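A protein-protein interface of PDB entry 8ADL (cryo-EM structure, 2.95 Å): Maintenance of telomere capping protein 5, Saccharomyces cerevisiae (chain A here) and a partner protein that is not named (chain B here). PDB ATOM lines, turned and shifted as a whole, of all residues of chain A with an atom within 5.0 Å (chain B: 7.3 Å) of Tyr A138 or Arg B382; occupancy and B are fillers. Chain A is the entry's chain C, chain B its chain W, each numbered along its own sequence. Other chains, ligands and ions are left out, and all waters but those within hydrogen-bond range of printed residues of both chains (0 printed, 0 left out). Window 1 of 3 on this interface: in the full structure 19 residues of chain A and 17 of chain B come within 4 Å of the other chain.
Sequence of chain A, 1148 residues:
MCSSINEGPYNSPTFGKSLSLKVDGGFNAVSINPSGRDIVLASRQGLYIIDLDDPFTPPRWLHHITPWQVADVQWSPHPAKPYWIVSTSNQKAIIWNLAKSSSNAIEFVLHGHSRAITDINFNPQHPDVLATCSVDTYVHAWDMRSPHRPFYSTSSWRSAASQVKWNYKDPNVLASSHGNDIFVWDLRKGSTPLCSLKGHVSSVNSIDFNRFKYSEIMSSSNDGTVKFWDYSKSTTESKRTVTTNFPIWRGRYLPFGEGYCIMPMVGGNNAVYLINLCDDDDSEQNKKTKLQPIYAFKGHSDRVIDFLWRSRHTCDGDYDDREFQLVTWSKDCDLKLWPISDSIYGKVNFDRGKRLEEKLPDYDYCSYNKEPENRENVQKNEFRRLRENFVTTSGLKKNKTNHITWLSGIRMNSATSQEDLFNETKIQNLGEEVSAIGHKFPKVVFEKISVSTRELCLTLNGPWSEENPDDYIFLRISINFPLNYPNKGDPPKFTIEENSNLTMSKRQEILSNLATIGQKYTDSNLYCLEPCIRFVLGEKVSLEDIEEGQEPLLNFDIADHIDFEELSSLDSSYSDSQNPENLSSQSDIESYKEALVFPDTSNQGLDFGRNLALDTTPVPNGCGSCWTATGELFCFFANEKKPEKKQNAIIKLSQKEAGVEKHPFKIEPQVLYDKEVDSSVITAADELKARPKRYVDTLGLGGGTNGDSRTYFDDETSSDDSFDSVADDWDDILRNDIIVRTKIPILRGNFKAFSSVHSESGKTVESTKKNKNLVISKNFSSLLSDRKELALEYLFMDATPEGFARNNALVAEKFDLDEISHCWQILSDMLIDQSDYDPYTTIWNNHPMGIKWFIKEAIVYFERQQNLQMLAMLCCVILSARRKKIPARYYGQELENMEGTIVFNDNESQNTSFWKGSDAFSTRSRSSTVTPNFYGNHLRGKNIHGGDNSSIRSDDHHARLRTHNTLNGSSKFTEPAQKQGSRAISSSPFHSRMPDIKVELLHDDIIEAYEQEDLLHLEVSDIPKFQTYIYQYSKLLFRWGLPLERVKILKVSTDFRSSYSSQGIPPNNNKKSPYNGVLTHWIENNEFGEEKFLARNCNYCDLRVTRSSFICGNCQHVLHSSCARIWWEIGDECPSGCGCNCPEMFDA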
ATOM      1  N   HIS A 113       8.733 -17.038  -3.971  1.00  0.00           N
ATOM      2  CA  HIS A 113       8.799 -15.959  -2.993  1.00  0.00           C
ATOM      3  C   HIS A 113      10.238 -15.702  -2.547  1.00  0.00           C
ATOM      4  O   HIS A 113      11.132 -16.536  -2.713  1.00  0.00           O
ATOM      5  CB  HIS A 113       7.939 -16.288  -1.771  1.00  0.00           C
ATOM      6  CG  HIS A 113       6.666 -17.006  -2.098  1.00  0.00           C
ATOM      7  ND1 HIS A 113       5.516 -16.348  -2.480  1.00  0.00           N
ATOM      8  CD2 HIS A 113       6.359 -18.325  -2.089  1.00  0.00           C
ATOM      9  CE1 HIS A 113       4.557 -17.231  -2.692  1.00  0.00           C
ATOM     10  NE2 HIS A 113       5.043 -18.438  -2.465  1.00  0.00           N
ATOM     11  N   THR A 132       0.918 -21.613  -2.872  1.00  0.00           N
ATOM     12  CA  THR A 132       1.889 -21.390  -1.810  1.00  0.00           C
ATOM     13  C   THR A 132       1.713 -19.990  -1.240  1.00  0.00           C
ATOM     14  O   THR A 132       1.561 -19.019  -1.987  1.00  0.00           O
ATOM     15  CB  THR A 132       3.334 -21.556  -2.311  1.00  0.00           C
ATOM     16  OG1 THR A 132       3.697 -20.428  -3.118  1.00  0.00           O
ATOM     17  CG2 THR A 132       3.490 -22.831  -3.127  1.00  0.00           C
ATOM     18  N   CYS A 133       1.739 -19.893   0.086  1.00  0.00           N
ATOM     19  CA  CYS A 133       1.706 -18.619   0.784  1.00  0.00           C
ATOM     20  C   CYS A 133       2.960 -18.495   1.639  1.00  0.00           C
ATOM     21  O   CYS A 133       3.567 -19.496   2.031  1.00  0.00           O
ATOM     22  CB  CYS A 133       0.446 -18.487   1.649  1.00  0.00           C
ATOM     23  SG  CYS A 133       0.546 -19.288   3.265  1.00  0.00           S
ATOM     24  N   SER A 134       3.352 -17.257   1.930  1.00  0.00           N
ATOM     25  CA  SER A 134       4.664 -17.026   2.513  1.00  0.00           C
ATOM     26  C   SER A 134       4.639 -15.796   3.410  1.00  0.00           C
ATOM     27  O   SER A 134       3.645 -15.071   3.487  1.00  0.00           O
ATOM     28  CB  SER A 134       5.720 -16.876   1.414  1.00  0.00           C
ATOM     29  OG  SER A 134       5.326 -15.896   0.472  1.00  0.00           O
ATOM     30  N   ASP A 136       6.532 -13.156   2.999  1.00  0.00           N
ATOM     31  CA  ASP A 136       6.776 -11.933   2.238  1.00  0.00           C
ATOM     32  C   ASP A 136       5.507 -11.320   1.629  1.00  0.00           C
ATOM     33  O   ASP A 136       5.630 -10.492   0.716  1.00  0.00           O
ATOM     34  CB  ASP A 136       7.818 -12.192   1.142  1.00  0.00           C
ATOM     35  CG  ASP A 136       7.283 -13.039   0.002  1.00  0.00           C
ATOM     36  OD1 ASP A 136       6.417 -13.902   0.245  1.00  0.00           O
ATOM     37  OD2 ASP A 136       7.733 -12.839  -1.146  1.00  0.00           O
ATOM     38  N   THR A 137       4.328 -11.698   2.138  1.00  0.00           N
ATOM     39  CA  THR A 137       3.018 -11.199   1.703  1.00  0.00           C
ATOM     40  C   THR A 137       2.795 -11.450   0.209  1.00  0.00           C
ATOM     41  O   THR A 137       2.637 -10.526  -0.591  1.00  0.00           O
ATOM     42  CB  THR A 137       2.828  -9.714   2.052  1.00  0.00           C
ATOM     43  OG1 THR A 137       3.582  -8.901   1.142  1.00  0.00           O
ATOM     44  CG2 THR A 137       3.268  -9.425   3.486  1.00  0.00           C
ATOM     45  N   TYR A 138       2.778 -12.732  -0.150  1.00  0.00           N
ATOM     46  CA  TYR A 138       2.503 -13.155  -1.514  1.00  0.00           C
ATOM     47  C   TYR A 138       1.855 -14.529  -1.481  1.00  0.00           C
ATOM     48  O   TYR A 138       2.256 -15.393  -0.697  1.00  0.00           O
ATOM     49  CB  TYR A 138       3.775 -13.201  -2.370  1.00  0.00           C
ATOM     50  CG  TYR A 138       4.187 -11.863  -2.936  1.00  0.00           C
ATOM     51  CD1 TYR A 138       3.539 -11.329  -4.042  1.00  0.00           C
ATOM     52  CD2 TYR A 138       5.226 -11.137  -2.369  1.00  0.00           C
ATOM     53  CE1 TYR A 138       3.909 -10.109  -4.563  1.00  0.00           C
ATOM     54  CE2 TYR A 138       5.603  -9.914  -2.883  1.00  0.00           C
ATOM     55  CZ  TYR A 138       4.942  -9.408  -3.981  1.00  0.00           C
ATOM     56  OH  TYR A 138       5.313  -8.194  -4.498  1.00  0.00           O
ATOM     57  N   VAL A 139       0.855 -14.722  -2.334  1.00  0.00           N
ATOM     58  CA  VAL A 139       0.245 -16.025  -2.564  1.00  0.00           C
ATOM     59  C   VAL A 139       0.436 -16.375  -4.033  1.00  0.00           C
ATOM     60  O   VAL A 139      -0.106 -15.695  -4.915  1.00  0.00           O
ATOM     61  CB  VAL A 139      -1.239 -16.047  -2.176  1.00  0.00           C
ATOM     62  CG1 VAL A 139      -1.897 -17.339  -2.647  1.00  0.00           C
ATOM     63  CG2 VAL A 139      -1.397 -15.876  -0.672  1.00  0.00           C
ATOM     64  N   HIS A 140       1.209 -17.422  -4.301  1.00  0.00           N
ATOM     65  CA  HIS A 140       1.513 -17.853  -5.658  1.00  0.00           C
ATOM     66  C   HIS A 140       0.825 -19.183  -5.922  1.00  0.00           C
ATOM     67  O   HIS A 140       0.908 -20.103  -5.102  1.00  0.00           O
ATOM     68  CB  HIS A 140       3.021 -17.987  -5.884  1.00  0.00           C
ATOM     69  CG  HIS A 140       3.732 -16.677  -6.016  1.00  0.00           C
ATOM     70  ND1 HIS A 140       3.090 -15.516  -6.394  1.00  0.00           N
ATOM     71  CD2 HIS A 140       5.033 -16.346  -5.841  1.00  0.00           C
ATOM     72  CE1 HIS A 140       3.963 -14.526  -6.433  1.00  0.00           C
ATOM     73  NE2 HIS A 140       5.149 -15.002  -6.100  1.00  0.00           N
ATOM     74  N   SER A 153      -0.555 -14.815  -9.415  1.00  0.00           N
ATOM     75  CA  SER A 153       0.091 -14.145  -8.296  1.00  0.00           C
ATOM     76  C   SER A 153      -0.859 -13.139  -7.665  1.00  0.00           C
ATOM     77  O   SER A 153      -1.535 -12.383  -8.369  1.00  0.00           O
ATOM     78  CB  SER A 153       1.376 -13.435  -8.739  1.00  0.00           C
ATOM     79  OG  SER A 153       1.758 -12.444  -7.801  1.00  0.00           O
ATOM     80  N   THR A 154      -0.907 -13.138  -6.334  1.00  0.00           N
ATOM     81  CA  THR A 154      -1.702 -12.169  -5.595  1.00  0.00           C
ATOM     82  C   THR A 154      -1.048 -11.900  -4.247  1.00  0.00           C
ATOM     83  O   THR A 154      -0.187 -12.656  -3.788  1.00  0.00           O
ATOM     84  CB  THR A 154      -3.145 -12.648  -5.403  1.00  0.00           C
ATOM     85  OG1 THR A 154      -3.919 -11.594  -4.822  1.00  0.00           O
ATOM     86  CG2 THR A 154      -3.196 -13.862  -4.493  1.00  0.00           C
ATOM     87  N   SER A 155      -1.463 -10.800  -3.621  1.00  0.00           N
ATOM     88  CA  SER A 155      -0.830 -10.329  -2.399  1.00  0.00           C
ATOM     89  C   SER A 155      -1.851  -9.583  -1.550  1.00  0.00           C
ATOM     90  O   SER A 155      -2.860  -9.080  -2.053  1.00  0.00           O
ATOM     91  CB  SER A 155       0.370  -9.424  -2.705  1.00  0.00           C
ATOM     92  OG  SER A 155       0.914  -8.877  -1.518  1.00  0.00           O
ATOM     93  N   TRP A 157      -0.315  -7.286   0.732  1.00  0.00           N
ATOM     94  CA  TRP A 157       0.532  -6.092   0.787  1.00  0.00           C
ATOM     95  C   TRP A 157       0.757  -5.527   2.189  1.00  0.00           C
ATOM     96  O   TRP A 157       1.542  -4.587   2.350  1.00  0.00           O
ATOM     97  CB  TRP A 157      -0.033  -4.983  -0.108  1.00  0.00           C
ATOM     98  CG  TRP A 157      -0.420  -5.429  -1.485  1.00  0.00           C
ATOM     99  CD1 TRP A 157      -1.688  -5.595  -1.962  1.00  0.00           C
ATOM    100  CD2 TRP A 157       0.461  -5.750  -2.568  1.00  0.00           C
ATOM    101  NE1 TRP A 157      -1.651  -6.006  -3.272  1.00  0.00           N
ATOM    102  CE2 TRP A 157      -0.344  -6.107  -3.669  1.00  0.00           C
ATOM    103  CE3 TRP A 157       1.851  -5.773  -2.714  1.00  0.00           C
ATOM    104  CZ2 TRP A 157       0.193  -6.485  -4.897  1.00  0.00           C
ATOM    105  CZ3 TRP A 157       2.384  -6.148  -3.936  1.00  0.00           C
ATOM    106  CH2 TRP A 157       1.555  -6.500  -5.010  1.00  0.00           C
ATOM    107  N   ILE B 285      14.436   3.180  -4.154  1.00  0.00           N
ATOM    108  CA  ILE B 285      13.681   1.954  -3.922  1.00  0.00           C
ATOM    109  C   ILE B 285      13.983   0.986  -5.060  1.00  0.00           C
ATOM    110  O   ILE B 285      13.659   1.250  -6.220  1.00  0.00           O
ATOM    111  CB  ILE B 285      12.177   2.227  -3.811  1.00  0.00           C
ATOM    112  CG1 ILE B 285      11.874   3.038  -2.547  1.00  0.00           C
ATOM    113  CG2 ILE B 285      11.397   0.915  -3.822  1.00  0.00           C
ATOM    114  CD1 ILE B 285      10.398   3.127  -2.208  1.00  0.00           C
ATOM    115  N   THR B 286      14.623  -0.132  -4.730  1.00  0.00           N
ATOM    116  CA  THR B 286      15.020  -1.134  -5.707  1.00  0.00           C
ATOM    117  C   THR B 286      14.667  -2.501  -5.136  1.00  0.00           C
ATOM    118  O   THR B 286      13.972  -2.612  -4.120  1.00  0.00           O
ATOM    119  CB  THR B 286      16.518  -1.041  -6.035  1.00  0.00           C
ATOM    120  OG1 THR B 286      17.275  -1.069  -4.821  1.00  0.00           O
ATOM    121  CG2 THR B 286      16.847   0.226  -6.824  1.00  0.00           C
ATOM    122  N   ASP B 287      15.150  -3.554  -5.795  1.00  0.00           N
ATOM    123  CA  ASP B 287      14.942  -4.905  -5.288  1.00  0.00           C
ATOM    124  C   ASP B 287      15.783  -5.185  -4.049  1.00  0.00           C
ATOM    125  O   ASP B 287      15.442  -6.085  -3.274  1.00  0.00           O
ATOM    126  CB  ASP B 287      15.259  -5.929  -6.379  1.00  0.00           C
ATOM    127  CG  ASP B 287      14.683  -7.299  -6.078  1.00  0.00           C
ATOM    128  OD1 ASP B 287      13.482  -7.513  -6.346  1.00  0.00           O
ATOM    129  OD2 ASP B 287      15.432  -8.163  -5.574  1.00  0.00           O
ATOM    130  N   TRP B 290      14.738  -4.659   0.244  1.00  0.00           N
ATOM    131  CA  TRP B 290      14.273  -5.767   1.063  1.00  0.00           C
ATOM    132  C   TRP B 290      15.270  -6.917   1.096  1.00  0.00           C
ATOM    133  O   TRP B 290      14.956  -7.986   1.629  1.00  0.00           O
ATOM    134  CB  TRP B 290      12.913  -6.252   0.559  1.00  0.00           C
ATOM    135  CG  TRP B 290      11.839  -5.213   0.679  1.00  0.00           C
ATOM    136  CD1 TRP B 290      11.018  -5.001   1.751  1.00  0.00           C
ATOM    137  CD2 TRP B 290      11.474  -4.238  -0.304  1.00  0.00           C
ATOM    138  NE1 TRP B 290      10.163  -3.957   1.492  1.00  0.00           N
ATOM    139  CE2 TRP B 290      10.422  -3.471   0.239  1.00  0.00           C
ATOM    140  CE3 TRP B 290      11.931  -3.939  -1.592  1.00  0.00           C
ATOM    141  CZ2 TRP B 290       9.823  -2.426  -0.461  1.00  0.00           C
ATOM    142  CZ3 TRP B 290      11.334  -2.899  -2.285  1.00  0.00           C
ATOM    143  CH2 TRP B 290      10.292  -2.156  -1.719  1.00  0.00           C
ATOM    144  N   GLU B 377       4.301   5.459   3.779  1.00  0.00           N
ATOM    145  CA  GLU B 377       4.434   5.429   2.329  1.00  0.00           C
ATOM    146  C   GLU B 377       5.353   4.306   1.868  1.00  0.00           C
ATOM    147  O   GLU B 377       5.129   3.734   0.798  1.00  0.00           O
ATOM    148  CB  GLU B 377       4.932   6.776   1.810  1.00  0.00           C
ATOM    149  CG  GLU B 377       3.906   7.894   1.930  1.00  0.00           C
ATOM    150  CD  GLU B 377       2.499   7.436   1.595  1.00  0.00           C
ATOM    151  OE1 GLU B 377       2.251   7.076   0.424  1.00  0.00           O
ATOM    152  OE2 GLU B 377       1.641   7.438   2.502  1.00  0.00           O
ATOM    153  N   PHE B 378       6.378   3.964   2.655  1.00  0.00           N
ATOM    154  CA  PHE B 378       7.205   2.819   2.292  1.00  0.00           C
ATOM    155  C   PHE B 378       6.448   1.507   2.450  1.00  0.00           C
ATOM    156  O   PHE B 378       6.682   0.565   1.685  1.00  0.00           O
ATOM    157  CB  PHE B 378       8.486   2.798   3.125  1.00  0.00           C
ATOM    158  CG  PHE B 378       9.611   2.037   2.479  1.00  0.00           C
ATOM    159  CD1 PHE B 378       9.755   0.672   2.679  1.00  0.00           C
ATOM    160  CD2 PHE B 378      10.523   2.691   1.665  1.00  0.00           C
ATOM    161  CE1 PHE B 378      10.787  -0.025   2.075  1.00  0.00           C
ATOM    162  CE2 PHE B 378      11.558   2.001   1.062  1.00  0.00           C
ATOM    163  CZ  PHE B 378      11.691   0.642   1.267  1.00  0.00           C
ATOM    164  N   MET B 379       5.547   1.416   3.432  1.00  0.00           N
ATOM    165  CA  MET B 379       4.727   0.214   3.540  1.00  0.00           C
ATOM    166  C   MET B 379       3.668   0.149   2.446  1.00  0.00           C
ATOM    167  O   MET B 379       3.258  -0.948   2.051  1.00  0.00           O
ATOM    168  CB  MET B 379       4.073   0.149   4.919  1.00  0.00           C
ATOM    169  CG  MET B 379       5.015  -0.279   6.032  1.00  0.00           C
ATOM    170  SD  MET B 379       5.610  -1.969   5.855  1.00  0.00           S
ATOM    171  CE  MET B 379       7.224  -1.834   6.621  1.00  0.00           C
ATOM    172  N   GLU B 380       3.216   1.300   1.944  1.00  0.00           N
ATOM    173  CA  GLU B 380       2.179   1.325   0.919  1.00  0.00           C
ATOM    174  C   GLU B 380       2.723   1.320  -0.506  1.00  0.00           C
ATOM    175  O   GLU B 380       1.938   1.131  -1.444  1.00  0.00           O
ATOM    176  CB  GLU B 380       1.283   2.553   1.110  1.00  0.00           C
ATOM    177  CG  GLU B 380       0.284   2.419   2.245  1.00  0.00           C
ATOM    178  CD  GLU B 380      -0.679   3.587   2.315  1.00  0.00           C
ATOM    179  OE1 GLU B 380      -0.633   4.451   1.415  1.00  0.00           O
ATOM    180  OE2 GLU B 380      -1.480   3.642   3.272  1.00  0.00           O
ATOM    181  N   ILE B 381       4.029   1.540  -0.687  1.00  0.00           N
ATOM    182  CA  ILE B 381       4.595   1.680  -2.026  1.00  0.00           C
ATOM    183  C   ILE B 381       4.533   0.361  -2.798  1.00  0.00           C
ATOM    184  O   ILE B 381       4.404   0.364  -4.030  1.00  0.00           O
ATOM    185  CB  ILE B 381       6.022   2.266  -1.931  1.00  0.00           C
ATOM    186  CG1 ILE B 381       6.424   2.938  -3.243  1.00  0.00           C
ATOM    187  CG2 ILE B 381       7.064   1.224  -1.526  1.00  0.00           C
ATOM    188  CD1 ILE B 381       5.643   4.195  -3.549  1.00  0.00           C
ATOM    189  N   ARG B 382       4.581  -0.779  -2.095  1.00  0.00           N
ATOM    190  CA  ARG B 382       4.514  -2.075  -2.765  1.00  0.00           C
ATOM    191  C   ARG B 382       3.133  -2.310  -3.361  1.00  0.00           C
ATOM    192  O   ARG B 382       3.011  -2.756  -4.507  1.00  0.00           O
ATOM    193  CB  ARG B 382       4.872  -3.190  -1.780  1.00  0.00           C
ATOM    194  CG  ARG B 382       6.296  -3.123  -1.245  1.00  0.00           C
ATOM    195  CD  ARG B 382       6.833  -4.499  -0.874  1.00  0.00           C
ATOM    196  NE  ARG B 382       7.580  -5.126  -1.957  1.00  0.00           N
ATOM    197  CZ  ARG B 382       7.950  -6.401  -1.973  1.00  0.00           C
ATOM    198  NH1 ARG B 382       7.657  -7.218  -0.975  1.00  0.00           N
ATOM    199  NH2 ARG B 382       8.631  -6.867  -3.016  1.00  0.00           N
ATOM    200  N   LYS B 383       2.080  -2.009  -2.596  1.00  0.00           N
ATOM    201  CA  LYS B 383       0.722  -2.066  -3.124  1.00  0.00           C
ATOM    202  C   LYS B 383       0.500  -1.019  -4.209  1.00  0.00           C
ATOM    203  O   LYS B 383      -0.240  -1.268  -5.169  1.00  0.00           O
ATOM    204  CB  LYS B 383      -0.284  -1.881  -1.987  1.00  0.00           C
ATOM    205  CG  LYS B 383      -1.738  -2.088  -2.376  1.00  0.00           C
ATOM    206  CD  LYS B 383      -2.668  -1.729  -1.228  1.00  0.00           C
ATOM    207  CE  LYS B 383      -3.974  -2.504  -1.313  1.00  0.00           C
ATOM    208  NZ  LYS B 383      -4.364  -2.793  -2.720  1.00  0.00           N
ATOM    209  N   ASP B 384       1.127   0.154  -4.068  1.00  0.00           N
ATOM    210  CA  ASP B 384       0.971   1.222  -5.051  1.00  0.00           C
ATOM    211  C   ASP B 384       1.563   0.846  -6.405  1.00  0.00           C
ATOM    212  O   ASP B 384       0.986   1.169  -7.450  1.00  0.00           O
ATOM    213  CB  ASP B 384       1.618   2.504  -4.528  1.00  0.00           C
ATOM    214  CG  ASP B 384       0.769   3.197  -3.485  1.00  0.00           C
ATOM    215  OD1 ASP B 384      -0.424   2.847  -3.360  1.00  0.00           O
ATOM    216  OD2 ASP B 384       1.296   4.086  -2.783  1.00  0.00           O
ATOM    217  N   LEU B 385       2.707   0.164  -6.413  1.00  0.00           N
ATOM    218  CA  LEU B 385       3.428  -0.083  -7.657  1.00  0.00           C
ATOM    219  C   LEU B 385       3.239  -1.486  -8.216  1.00  0.00           C
ATOM    220  O   LEU B 385       3.028  -1.637  -9.423  1.00  0.00           O
ATOM    221  CB  LEU B 385       4.922   0.171  -7.456  1.00  0.00           C
ATOM    222  CG  LEU B 385       5.302   1.627  -7.226  1.00  0.00           C
ATOM    223  CD1 LEU B 385       6.687   1.695  -6.649  1.00  0.00           C
ATOM    224  CD2 LEU B 385       5.239   2.372  -8.542  1.00  0.00           C
ATOM    225  N   LEU B 386       3.306  -2.515  -7.380  1.00  0.00           N
ATOM    226  CA  LEU B 386       3.303  -3.887  -7.862  1.00  0.00           C
ATOM    227  C   LEU B 386       1.900  -4.435  -8.092  1.00  0.00           C
ATOM    228  O   LEU B 386       1.760  -5.610  -8.446  1.00  0.00           O
ATOM    229  CB  LEU B 386       4.068  -4.777  -6.877  1.00  0.00           C
ATOM    230  CG  LEU B 386       5.543  -4.394  -6.710  1.00  0.00           C
ATOM    231  CD1 LEU B 386       6.263  -5.358  -5.787  1.00  0.00           C
ATOM    232  CD2 LEU B 386       6.240  -4.337  -8.056  1.00  0.00           C
ATOM    233  N   ASN B 387       0.866  -3.623  -7.892  1.00  0.00           N
ATOM    234  CA  ASN B 387      -0.518  -3.998  -8.172  1.00  0.00           C
ATOM    235  C   ASN B 387      -1.018  -3.129  -9.323  1.00  0.00           C
ATOM    236  O   ASN B 387      -1.630  -2.082  -9.108  1.00  0.00           O
ATOM    237  CB  ASN B 387      -1.396  -3.839  -6.934  1.00  0.00           C
ATOM    238  CG  ASN B 387      -2.368  -4.989  -6.758  1.00  0.00           C
ATOM    239  OD1 ASN B 387      -2.089  -6.120  -7.158  1.00  0.00           O
ATOM    240  ND2 ASN B 387      -3.518  -4.704  -6.161  1.00  0.00           N
ATOM    241  N   LYS B 388      -0.754  -3.569 -10.550  1.00  0.00           N
ATOM    242  CA  LYS B 388      -1.184  -2.818 -11.718  1.00  0.00           C
ATOM    243  C   LYS B 388      -2.674  -3.022 -11.957  1.00  0.00           C
ATOM    244  O   LYS B 388      -3.265  -4.021 -11.533  1.00  0.00           O
ATOM    245  CB  LYS B 388      -0.397  -3.232 -12.965  1.00  0.00           C
ATOM    246  CG  LYS B 388      -0.815  -4.568 -13.563  1.00  0.00           C
ATOM    247  CD  LYS B 388      -0.038  -4.892 -14.823  1.00  0.00           C
ATOM    248  CE  LYS B 388      -0.631  -6.102 -15.528  1.00  0.00           C
ATOM    249  NZ  LYS B 388       0.107  -6.442 -16.775  1.00  0.00           N
ATOM    250  N   ALA B 397      -1.273  -8.569  -9.898  1.00  0.00           N
ATOM    251  CA  ALA B 397      -0.013  -8.364  -9.187  1.00  0.00           C
ATOM    252  C   ALA B 397       1.132  -8.559 -10.173  1.00  0.00           C
ATOM    253  O   ALA B 397       1.571  -9.684 -10.422  1.00  0.00           O
ATOM    254  CB  ALA B 397       0.100  -9.321  -8.007  1.00  0.00           C
ATOM    255  N   ASN B 398       1.625  -7.458 -10.737  1.00  0.00           N
ATOM    256  CA  ASN B 398       2.658  -7.505 -11.759  1.00  0.00           C
ATOM    257  C   ASN B 398       3.645  -6.367 -11.540  1.00  0.00           C
ATOM    258  O   ASN B 398       3.346  -5.375 -10.871  1.00  0.00           O
ATOM    259  CB  ASN B 398       2.059  -7.422 -13.170  1.00  0.00           C
ATOM    260  CG  ASN B 398       2.952  -8.046 -14.224  1.00  0.00           C
ATOM    261  OD1 ASN B 398       3.888  -8.779 -13.905  1.00  0.00           O
ATOM    262  ND2 ASN B 398       2.671  -7.751 -15.488  1.00  0.00           N
ATOM    263  N   GLY B 399       4.820  -6.524 -12.118  1.00  0.00           N
ATOM    264  CA  GLY B 399       5.870  -5.534 -12.021  1.00  0.00           C
ATOM    265  C   GLY B 399       7.007  -6.019 -11.139  1.00  0.00           C
ATOM    266  O   GLY B 399       6.828  -6.861 -10.247  1.00  0.00           O
ATOM    267  N   PHE B 401      10.836  -4.475  -9.290  1.00  0.00           N
ATOM    268  CA  PHE B 401      11.801  -3.409  -9.063  1.00  0.00           C
ATOM    269  C   PHE B 401      13.112  -3.722  -9.771  1.00  0.00           C
ATOM    270  O   PHE B 401      13.567  -4.870  -9.795  1.00  0.00           O
ATOM    271  CB  PHE B 401      12.051  -3.225  -7.567  1.00  0.00           C
ATOM    272  CG  PHE B 401      10.841  -2.782  -6.793  1.00  0.00           C
ATOM    273  CD1 PHE B 401      10.289  -1.527  -7.000  1.00  0.00           C
ATOM    274  CD2 PHE B 401      10.265  -3.617  -5.846  1.00  0.00           C
ATOM    275  CE1 PHE B 401       9.179  -1.116  -6.284  1.00  0.00           C
ATOM    276  CE2 PHE B 401       9.154  -3.212  -5.126  1.00  0.00           C
ATOM    277  CZ  PHE B 401       8.610  -1.960  -5.345  1.00  0.00           C
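Of the printed residues of chain B, Tyr A138 touches Arg B382 (3.9 Å) and Leu B386 (3.3 Å). Arg B382 touches two residues of chain A. Printed residues of chain A within 4 Å of Leu B386: Tyr A138 (3.3 Å) and Trp A157 (3.6 Å). Of the printed residues of chain A, Lys B383 touches Trp A157. Of the printed residues of chain A, Asn B387 touches Trp A157. Thr A137 touches none of the printed residues of chain B. The nearest residue of chain B that does not touch Tyr A138 is Ala B397 (5.2 Å). The nearest printed residue of chain A that does not touch Lys B383 is Ser A155 (6.5 Å).
Of the 20 printed residues of chain B, 5 touch a printed residue of chain A. Printed residues of chain A that touch a printed residue of chain B: Tyr A138, Ser A153 and Trp A157. Among the printed residues, 7 pairs touch across the chains.
The backbone carbonyl oxygen of Leu B386 sits at hydrogen-bond distance from the backbone NH of Asn B398 (2.9 Å). OG of Ser A155 is in hydrogen-bond range of N of Trp A157 (3.0 Å). OG of Ser A134 sits at hydrogen-bond distance from O of Tyr A138 (3.3 Å).
Among the printed residues, pairs that only touch across the chains: Tyr A138 with Arg B382, Tyr A138 with Leu B386, Ser A153 with Ala B397, Trp A157 with Arg B382, Trp A157 with Lys B383, Trp A157 with Leu B386 and Trp A157 with Asn B387.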
